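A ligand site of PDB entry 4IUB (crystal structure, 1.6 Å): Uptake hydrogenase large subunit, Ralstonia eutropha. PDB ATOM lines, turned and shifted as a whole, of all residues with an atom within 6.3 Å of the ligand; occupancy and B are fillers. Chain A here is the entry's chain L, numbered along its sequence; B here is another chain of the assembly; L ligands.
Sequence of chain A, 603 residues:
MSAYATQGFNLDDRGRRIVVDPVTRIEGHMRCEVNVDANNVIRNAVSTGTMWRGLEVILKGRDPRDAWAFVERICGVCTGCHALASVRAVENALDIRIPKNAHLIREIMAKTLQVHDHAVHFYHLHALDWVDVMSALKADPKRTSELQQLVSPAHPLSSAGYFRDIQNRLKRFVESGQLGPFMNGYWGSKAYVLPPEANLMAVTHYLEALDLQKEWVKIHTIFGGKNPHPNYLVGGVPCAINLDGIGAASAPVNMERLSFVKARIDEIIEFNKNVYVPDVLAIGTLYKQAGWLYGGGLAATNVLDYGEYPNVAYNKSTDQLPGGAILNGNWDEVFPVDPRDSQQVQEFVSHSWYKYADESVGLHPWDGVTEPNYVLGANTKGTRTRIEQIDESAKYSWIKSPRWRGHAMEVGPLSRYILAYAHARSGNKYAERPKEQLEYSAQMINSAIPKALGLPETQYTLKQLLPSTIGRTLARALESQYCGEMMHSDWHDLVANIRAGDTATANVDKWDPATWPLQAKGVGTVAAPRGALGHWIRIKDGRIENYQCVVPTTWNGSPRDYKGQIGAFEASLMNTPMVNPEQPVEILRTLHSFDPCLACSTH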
ATOM      1  N   GLU A  27      28.979  -9.975 -16.726  1.00  0.00           N
ATOM      2  CA  GLU A  27      29.346  -8.905 -15.806  1.00  0.00           C
ATOM      3  C   GLU A  27      29.067  -9.420 -14.402  1.00  0.00           C
ATOM      4  O   GLU A  27      28.011 -10.024 -14.146  1.00  0.00           O
ATOM      5  CB  GLU A  27      28.551  -7.619 -16.068  1.00  0.00           C
ATOM      6  CG  GLU A  27      29.010  -6.406 -15.255  1.00  0.00           C
ATOM      7  CD  GLU A  27      28.755  -6.541 -13.755  1.00  0.00           C
ATOM      8  OE1 GLU A  27      27.736  -7.158 -13.395  1.00  0.00           O
ATOM      9  OE2 GLU A  27      29.580  -6.041 -12.948  1.00  0.00           O
ATOM     10  N   ILE A  74      25.650   1.404 -10.527  1.00  0.00           N
ATOM     11  CA  ILE A  74      25.192   0.017 -10.439  1.00  0.00           C
ATOM     12  C   ILE A  74      25.918  -0.807 -11.495  1.00  0.00           C
ATOM     13  O   ILE A  74      26.216  -1.986 -11.277  1.00  0.00           O
ATOM     14  CB  ILE A  74      23.662  -0.093 -10.609  1.00  0.00           C
ATOM     15  CG1 ILE A  74      22.979   0.411  -9.329  1.00  0.00           C
ATOM     16  CG2 ILE A  74      23.250  -1.537 -10.919  1.00  0.00           C
ATOM     17  CD1 ILE A  74      21.472   0.570  -9.449  1.00  0.00           C
ATOM     18  N   CYS A  75      26.215  -0.191 -12.638  1.00  0.00           N
ATOM     19  CA  CYS A  75      26.797  -0.971 -13.736  1.00  0.00           C
ATOM     20  C   CYS A  75      27.485  -0.126 -14.773  1.00  0.00           C
ATOM     21  O   CYS A  75      26.913   0.832 -15.287  1.00  0.00           O
ATOM     22  CB  CYS A  75      25.702  -1.788 -14.406  1.00  0.00           C
ATOM     23  SG  CYS A  75      26.406  -2.980 -15.554  1.00  0.00           S
ATOM     24  N   GLY A  76      28.718  -0.516 -15.110  1.00  0.00           N
ATOM     25  CA  GLY A  76      29.529   0.185 -16.112  1.00  0.00           C
ATOM     26  C   GLY A  76      29.431  -0.451 -17.489  1.00  0.00           C
ATOM     27  O   GLY A  76      30.001   0.070 -18.453  1.00  0.00           O
ATOM     28  N   VAL A  77      28.716  -1.563 -17.598  1.00  0.00           N
ATOM     29  CA  VAL A  77      28.490  -2.220 -18.888  1.00  0.00           C
ATOM     30  C   VAL A  77      27.239  -1.596 -19.523  1.00  0.00           C
ATOM     31  O   VAL A  77      27.309  -1.031 -20.612  1.00  0.00           O
ATOM     32  CB  VAL A  77      28.339  -3.753 -18.756  1.00  0.00           C
ATOM     33  CG1 VAL A  77      28.135  -4.404 -20.118  1.00  0.00           C
ATOM     34  CG2 VAL A  77      29.568  -4.333 -18.063  1.00  0.00           C
ATOM     35  N   CYS A  78      26.107  -1.687 -18.826  1.00  0.00           N
ATOM     36  CA  CYS A  78      24.911  -0.978 -19.261  1.00  0.00           C
ATOM     37  C   CYS A  78      24.963   0.466 -18.756  1.00  0.00           C
ATOM     38  O   CYS A  78      24.020   0.997 -18.143  1.00  0.00           O
ATOM     39  CB  CYS A  78      23.625  -1.697 -18.832  1.00  0.00           C
ATOM     40  SG  CYS A  78      23.450  -1.969 -17.042  1.00  0.00           S
ATOM     41  N   THR A  79      26.080   1.117 -19.051  1.00  0.00           N
ATOM     42  CA  THR A  79      26.385   2.408 -18.473  1.00  0.00           C
ATOM     43  C   THR A  79      25.456   3.524 -18.954  1.00  0.00           C
ATOM     44  O   THR A  79      25.328   3.758 -20.160  1.00  0.00           O
ATOM     45  CB  THR A  79      27.873   2.785 -18.657  1.00  0.00           C
ATOM     46  OG1 THR A  79      28.105   4.024 -17.983  1.00  0.00           O
ATOM     47  CG2 THR A  79      28.243   2.937 -20.142  1.00  0.00           C
ATOM     48  N   CYS A  81      22.075   3.653 -18.412  1.00  0.00           N
ATOM     49  CA  CYS A  81      20.657   3.303 -18.422  1.00  0.00           C
ATOM     50  C   CYS A  81      20.040   3.536 -17.043  1.00  0.00           C
ATOM     51  O   CYS A  81      18.889   3.959 -16.928  1.00  0.00           O
ATOM     52  CB  CYS A  81      20.407   1.886 -18.979  1.00  0.00           C
ATOM     53  SG  CYS A  81      20.815   0.516 -17.872  1.00  0.00           S
ATOM     54  N   HIS A  82      20.824   3.309 -15.981  1.00  0.00           N
ATOM     55  CA  HIS A  82      20.355   3.613 -14.625  1.00  0.00           C
ATOM     56  C   HIS A  82      20.255   5.093 -14.368  1.00  0.00           C
ATOM     57  O   HIS A  82      19.372   5.526 -13.626  1.00  0.00           O
ATOM     58  CB  HIS A  82      21.260   2.973 -13.590  1.00  0.00           C
ATOM     59  CG  HIS A  82      21.108   1.482 -13.511  1.00  0.00           C
ATOM     60  ND1 HIS A  82      20.020   0.889 -12.969  1.00  0.00           N
ATOM     61  CD2 HIS A  82      21.948   0.462 -13.919  1.00  0.00           C
ATOM     62  CE1 HIS A  82      20.159  -0.434 -13.025  1.00  0.00           C
ATOM     63  NE2 HIS A  82      21.337  -0.712 -13.620  1.00  0.00           N
ATOM     64  N   LEU A 113      24.047   3.063 -26.352  1.00  0.00           N
ATOM     65  CA  LEU A 113      24.316   2.002 -25.368  1.00  0.00           C
ATOM     66  C   LEU A 113      23.814   0.649 -25.879  1.00  0.00           C
ATOM     67  O   LEU A 113      24.515  -0.358 -25.762  1.00  0.00           O
ATOM     68  CB  LEU A 113      23.688   2.329 -24.009  1.00  0.00           C
ATOM     69  CG  LEU A 113      23.848   1.242 -22.938  1.00  0.00           C
ATOM     70  CD1 LEU A 113      25.335   1.052 -22.614  1.00  0.00           C
ATOM     71  CD2 LEU A 113      23.050   1.575 -21.690  1.00  0.00           C
ATOM     72  N   ASP A 117      26.558  -2.181 -26.158  1.00  0.00           N
ATOM     73  CA  ASP A 117      26.346  -3.303 -25.251  1.00  0.00           C
ATOM     74  C   ASP A 117      26.056  -4.588 -26.021  1.00  0.00           C
ATOM     75  O   ASP A 117      26.656  -5.632 -25.768  1.00  0.00           O
ATOM     76  CB  ASP A 117      25.173  -2.933 -24.322  1.00  0.00           C
ATOM     77  CG  ASP A 117      25.259  -3.609 -22.973  1.00  0.00           C
ATOM     78  OD1 ASP A 117      25.758  -4.761 -22.916  1.00  0.00           O
ATOM     79  OD2 ASP A 117      24.819  -2.988 -21.977  1.00  0.00           O
ATOM     80  N   ALA A 528      16.207  -1.154 -21.084  1.00  0.00           N
ATOM     81  CA  ALA A 528      17.645  -1.303 -20.974  1.00  0.00           C
ATOM     82  C   ALA A 528      18.097  -2.458 -21.876  1.00  0.00           C
ATOM     83  O   ALA A 528      17.280  -3.292 -22.272  1.00  0.00           O
ATOM     84  CB  ALA A 528      18.031  -1.554 -19.526  1.00  0.00           C
ATOM     85  N   PRO A 529      19.396  -2.519 -22.206  1.00  0.00           N
ATOM     86  CA  PRO A 529      19.860  -3.567 -23.114  1.00  0.00           C
ATOM     87  C   PRO A 529      19.412  -4.985 -22.735  1.00  0.00           C
ATOM     88  O   PRO A 529      19.141  -5.783 -23.636  1.00  0.00           O
ATOM     89  CB  PRO A 529      21.377  -3.433 -23.065  1.00  0.00           C
ATOM     90  CG  PRO A 529      21.582  -1.959 -22.875  1.00  0.00           C
ATOM     91  CD  PRO A 529      20.464  -1.518 -21.940  1.00  0.00           C
ATOM     92  N   ARG A 530      19.301  -5.282 -21.436  1.00  0.00           N
ATOM     93  CA  ARG A 530      18.947  -6.634 -20.997  1.00  0.00           C
ATOM     94  C   ARG A 530      17.470  -6.847 -20.679  1.00  0.00           C
ATOM     95  O   ARG A 530      17.055  -7.957 -20.326  1.00  0.00           O
ATOM     96  CB  ARG A 530      19.823  -7.057 -19.806  1.00  0.00           C
ATOM     97  CG  ARG A 530      21.256  -7.316 -20.231  1.00  0.00           C
ATOM     98  CD  ARG A 530      22.254  -7.091 -19.099  1.00  0.00           C
ATOM     99  NE  ARG A 530      23.612  -7.182 -19.652  1.00  0.00           N
ATOM    100  CZ  ARG A 530      24.259  -6.156 -20.217  1.00  0.00           C
ATOM    101  NH1 ARG A 530      23.708  -4.953 -20.260  1.00  0.00           N
ATOM    102  NH2 ARG A 530      25.473  -6.347 -20.712  1.00  0.00           N
ATOM    103  N   GLY A 531      16.667  -5.791 -20.833  1.00  0.00           N
ATOM    104  CA  GLY A 531      15.225  -5.894 -20.647  1.00  0.00           C
ATOM    105  C   GLY A 531      14.601  -4.738 -19.888  1.00  0.00           C
ATOM    106  O   GLY A 531      15.013  -3.581 -20.030  1.00  0.00           O
ATOM    107  N   LEU A 533      13.814  -2.234 -17.166  1.00  0.00           N
ATOM    108  CA  LEU A 533      14.388  -1.585 -15.999  1.00  0.00           C
ATOM    109  C   LEU A 533      13.410  -0.577 -15.396  1.00  0.00           C
ATOM    110  O   LEU A 533      12.779   0.182 -16.111  1.00  0.00           O
ATOM    111  CB  LEU A 533      15.694  -0.866 -16.396  1.00  0.00           C
ATOM    112  CG  LEU A 533      16.329   0.079 -15.361  1.00  0.00           C
ATOM    113  CD1 LEU A 533      16.816  -0.694 -14.130  1.00  0.00           C
ATOM    114  CD2 LEU A 533      17.473   0.886 -15.974  1.00  0.00           C
ATOM    115  N   HIS A 535      13.101   2.232 -11.837  1.00  0.00           N
ATOM    116  CA  HIS A 535      13.511   2.838 -10.571  1.00  0.00           C
ATOM    117  C   HIS A 535      12.297   3.488  -9.970  1.00  0.00           C
ATOM    118  O   HIS A 535      11.629   4.268 -10.636  1.00  0.00           O
ATOM    119  CB  HIS A 535      14.554   3.936 -10.792  1.00  0.00           C
ATOM    120  CG  HIS A 535      15.929   3.441 -11.168  1.00  0.00           C
ATOM    121  ND1 HIS A 535      17.030   4.199 -10.991  1.00  0.00           N
ATOM    122  CD2 HIS A 535      16.377   2.238 -11.726  1.00  0.00           C
ATOM    123  CE1 HIS A 535      18.117   3.539 -11.411  1.00  0.00           C
ATOM    124  NE2 HIS A 535      17.726   2.337 -11.869  1.00  0.00           N
ATOM    125  N   VAL A 551      15.675  -4.572 -11.870  1.00  0.00           N
ATOM    126  CA  VAL A 551      16.594  -4.453 -12.996  1.00  0.00           C
ATOM    127  C   VAL A 551      16.418  -5.685 -13.888  1.00  0.00           C
ATOM    128  O   VAL A 551      15.964  -6.726 -13.409  1.00  0.00           O
ATOM    129  CB  VAL A 551      18.021  -4.271 -12.420  1.00  0.00           C
ATOM    130  CG1 VAL A 551      19.055  -3.984 -13.478  1.00  0.00           C
ATOM    131  CG2 VAL A 551      18.030  -3.145 -11.376  1.00  0.00           C
ATOM    132  N   PRO A 552      16.746  -5.578 -15.204  1.00  0.00           N
ATOM    133  CA  PRO A 552      16.407  -6.705 -16.067  1.00  0.00           C
ATOM    134  C   PRO A 552      16.973  -8.054 -15.592  1.00  0.00           C
ATOM    135  O   PRO A 552      16.246  -9.065 -15.592  1.00  0.00           O
ATOM    136  CB  PRO A 552      17.020  -6.304 -17.422  1.00  0.00           C
ATOM    137  CG  PRO A 552      16.966  -4.814 -17.406  1.00  0.00           C
ATOM    138  CD  PRO A 552      17.172  -4.398 -15.968  1.00  0.00           C
ATOM    139  N   THR A 553      18.246  -8.084 -15.192  1.00  0.00           N
ATOM    140  CA  THR A 553      18.828  -9.353 -14.733  1.00  0.00           C
ATOM    141  C   THR A 553      18.258  -9.791 -13.365  1.00  0.00           C
ATOM    142  O   THR A 553      18.307 -10.977 -13.013  1.00  0.00           O
ATOM    143  CB  THR A 553      20.378  -9.311 -14.788  1.00  0.00           C
ATOM    144  OG1 THR A 553      20.780  -8.941 -16.112  1.00  0.00           O
ATOM    145  CG2 THR A 553      21.002 -10.686 -14.483  1.00  0.00           C
ATOM    146  N   THR A 554      17.650  -8.861 -12.622  1.00  0.00           N
ATOM    147  CA  THR A 554      16.885  -9.269 -11.440  1.00  0.00           C
ATOM    148  C   THR A 554      15.739 -10.172 -11.889  1.00  0.00           C
ATOM    149  O   THR A 554      15.505 -11.224 -11.290  1.00  0.00           O
ATOM    150  CB  THR A 554      16.290  -8.078 -10.666  1.00  0.00           C
ATOM    151  OG1 THR A 554      17.257  -7.031 -10.558  1.00  0.00           O
ATOM    152  CG2 THR A 554      15.828  -8.534  -9.265  1.00  0.00           C
ATOM    153  N   ASP A 595      22.634 -12.430 -21.568  1.00  0.00           N
ATOM    154  CA  ASP A 595      23.584 -11.355 -21.317  1.00  0.00           C
ATOM    155  C   ASP A 595      23.537 -10.971 -19.821  1.00  0.00           C
ATOM    156  O   ASP A 595      23.233  -9.830 -19.467  1.00  0.00           O
ATOM    157  CB  ASP A 595      23.203 -10.190 -22.252  1.00  0.00           C
ATOM    158  CG  ASP A 595      24.125  -9.010 -22.147  1.00  0.00           C
ATOM    159  OD1 ASP A 595      25.211  -9.097 -21.551  1.00  0.00           O
ATOM    160  OD2 ASP A 595      23.714  -7.965 -22.692  1.00  0.00           O
ATOM    161  N   PRO A 596      23.815 -11.945 -18.934  1.00  0.00           N
ATOM    162  CA  PRO A 596      23.651 -11.640 -17.513  1.00  0.00           C
ATOM    163  C   PRO A 596      24.531 -10.488 -17.016  1.00  0.00           C
ATOM    164  O   PRO A 596      25.741 -10.482 -17.270  1.00  0.00           O
ATOM    165  CB  PRO A 596      24.068 -12.945 -16.826  1.00  0.00           C
ATOM    166  CG  PRO A 596      23.830 -13.993 -17.855  1.00  0.00           C
ATOM    167  CD  PRO A 596      24.229 -13.335 -19.147  1.00  0.00           C
ATOM    168  N   CYS A 597      23.917  -9.542 -16.314  1.00  0.00           N
ATOM    169  CA  CYS A 597      24.679  -8.506 -15.642  1.00  0.00           C
ATOM    170  C   CYS A 597      24.386  -8.629 -14.155  1.00  0.00           C
ATOM    171  O   CYS A 597      23.303  -8.249 -13.681  1.00  0.00           O
ATOM    172  CB  CYS A 597      24.305  -7.123 -16.148  1.00  0.00           C
ATOM    173  SG  CYS A 597      25.382  -5.846 -15.471  1.00  0.00           S
ATOM    174  N   LEU A 598      25.329  -9.206 -13.418  1.00  0.00           N
ATOM    175  CA  LEU A 598      25.038  -9.578 -12.025  1.00  0.00           C
ATOM    176  C   LEU A 598      25.109  -8.403 -11.064  1.00  0.00           C
ATOM    177  O   LEU A 598      24.366  -8.368 -10.080  1.00  0.00           O
ATOM    178  CB  LEU A 598      25.947 -10.744 -11.585  1.00  0.00           C
ATOM    179  CG  LEU A 598      25.414 -12.134 -11.955  1.00  0.00           C
ATOM    180  CD1 LEU A 598      24.278 -12.530 -11.003  1.00  0.00           C
ATOM    181  CD2 LEU A 598      24.965 -12.245 -13.406  1.00  0.00           C
ATOM    182  N   ALA A 599      25.974  -7.436 -11.353  1.00  0.00           N
ATOM    183  CA  ALA A 599      25.984  -6.176 -10.593  1.00  0.00           C
ATOM    184  C   ALA A 599      24.640  -5.470 -10.750  1.00  0.00           C
ATOM    185  O   ALA A 599      24.070  -4.987  -9.768  1.00  0.00           O
ATOM    186  CB  ALA A 599      27.134  -5.277 -11.039  1.00  0.00           C
ATOM    187  N   CYS A 600      24.108  -5.418 -11.971  1.00  0.00           N
ATOM    188  CA  CYS A 600      22.745  -4.913 -12.176  1.00  0.00           C
ATOM    189  C   CYS A 600      21.708  -5.682 -11.368  1.00  0.00           C
ATOM    190  O   CYS A 600      20.821  -5.081 -10.770  1.00  0.00           O
ATOM    191  CB  CYS A 600      22.359  -5.014 -13.648  1.00  0.00           C
ATOM    192  SG  CYS A 600      22.682  -3.499 -14.560  1.00  0.00           S
ATOM    193  N   SER A 601      21.806  -7.007 -11.398  1.00  0.00           N
ATOM    194  CA  SER A 601      20.730  -7.837 -10.824  1.00  0.00           C
ATOM    195  C   SER A 601      20.560  -7.605  -9.325  1.00  0.00           C
ATOM    196  O   SER A 601      19.449  -7.710  -8.788  1.00  0.00           O
ATOM    197  CB  SER A 601      20.964  -9.312 -11.104  1.00  0.00           C
ATOM    198  OG  SER A 601      22.019  -9.835 -10.302  1.00  0.00           O
ATOM    199  N   CYS B  17      31.289  -2.477 -10.546  1.00  0.00           N
ATOM    200  CA  CYS B  17      30.286  -2.269 -11.581  1.00  0.00           C
ATOM    201  C   CYS B  17      30.858  -2.621 -12.967  1.00  0.00           C
ATOM    202  O   CYS B  17      30.115  -2.636 -13.953  1.00  0.00           O
ATOM    203  CB  CYS B  17      29.763  -0.830 -11.571  1.00  0.00           C
ATOM    204  SG  CYS B  17      30.747   0.323 -12.543  1.00  0.00           S
HETATM  205 FE1  LIG L   1      21.755  -3.603 -16.717  1.00  0.00          FE
HETATM  206 NI1  LIG L   1      24.588  -3.941 -16.298  1.00  0.00          NI
HETATM  207  C1  LIG L   1      20.365  -2.522 -16.238  1.00  0.00           C
HETATM  208  O1  LIG L   1      19.476  -1.804 -15.960  1.00  0.00           O
HETATM  209  C2  LIG L   1      21.080  -3.646 -18.525  1.00  0.00           C
HETATM  210  N1  LIG L   1      20.693  -3.669 -19.579  1.00  0.00           N
HETATM  211  C3  LIG L   1      20.764  -5.227 -16.299  1.00  0.00           C
HETATM  212  N2  LIG L   1      20.202  -6.163 -16.048  1.00  0.00           N
HETATM  213  O2  LIG L   1      23.238  -4.832 -17.301  1.00  0.00           O
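SG of Cys 75 sits close to N of Val 77, 3.4 Å away.
NE2 of His 535 is in hydrogen-bond range of ND1 of His 82.
NH2 of Arg 530 is in salt-bridge range of OD1 of Asp 117 (2.7 Å).
NE2 of His 82 lies close to SG of Cys 600.
NH2 of Arg 530 lies within salt-bridge range of OD1 of Asp 595.
SG of Cys 597 sits close to OE1 of Glu 27 (3.4 Å).
The side-chain sulfur (SG) of Cys 81 lies within hydrogen-bond range of the backbone carbonyl oxygen (O) of Cys 78 (3.3 Å).
The backbone carbonyl oxygen (O) of Val 551 sits close to the side-chain hydroxyl (OG1) of Thr 554 (3.1 Å).
The backbone NH (N) of Arg 530 is in hydrogen-bond range of a nitrogen (N1) of the ligand.
SG of Cys 597 binds NI1 of the ligand, at 2.2 Å.
SG of Cys 78 is bound to FE1 of the ligand, at 2.4 Å.
The guanidinium group (NH1) of Arg 530 lies within hydrogen-bond range of a nitrogen (N1) of the ligand (3.3 Å).
N2 of the ligand lies within hydrogen-bond range of OG1 of Thr 553, 2.8 Å away.
NE2 of His 82 sits at hydrogen-bond distance from O1 of the ligand.
SG of Cys 75 binds NI1 of the ligand.
The side-chain sulfur (SG) of Cys 600 is bound to an iron atom (FE1) of the ligand, at 2.4 Å.
O1 of the ligand lies within hydrogen-bond range of SG of Cys 81 (3.3 Å).
The backbone NH of Thr 553 lies within hydrogen-bond range of a nitrogen (N2) of the ligand, at 2.9 Å.
N of Pro 529 sits close to N1 of the ligand, at 3.1 Å.
Ala 528 touches the ligand (CB to N1, 3.4 Å).
CD2 of Leu 533 touches O1 of the ligand, at 3.4 Å.
Val 551 touches the ligand (CG1 to O1, 3.3 Å).
Pro 552 touches the ligand (CB to N2, 3.5 Å).
Hydrophobic or aromatic side chains that line the ligand: His 82, Ala 528, Pro 529, Leu 533, Val 551 and Pro 552.
13 residues have an atom within 4 Å of the ligand: Cys 75, Cys 78, Cys 81, His 82, Ala 528, Pro 529, Arg 530, Leu 533, Val 551, Pro 552, Thr 553, Cys 597 and Cys 600.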
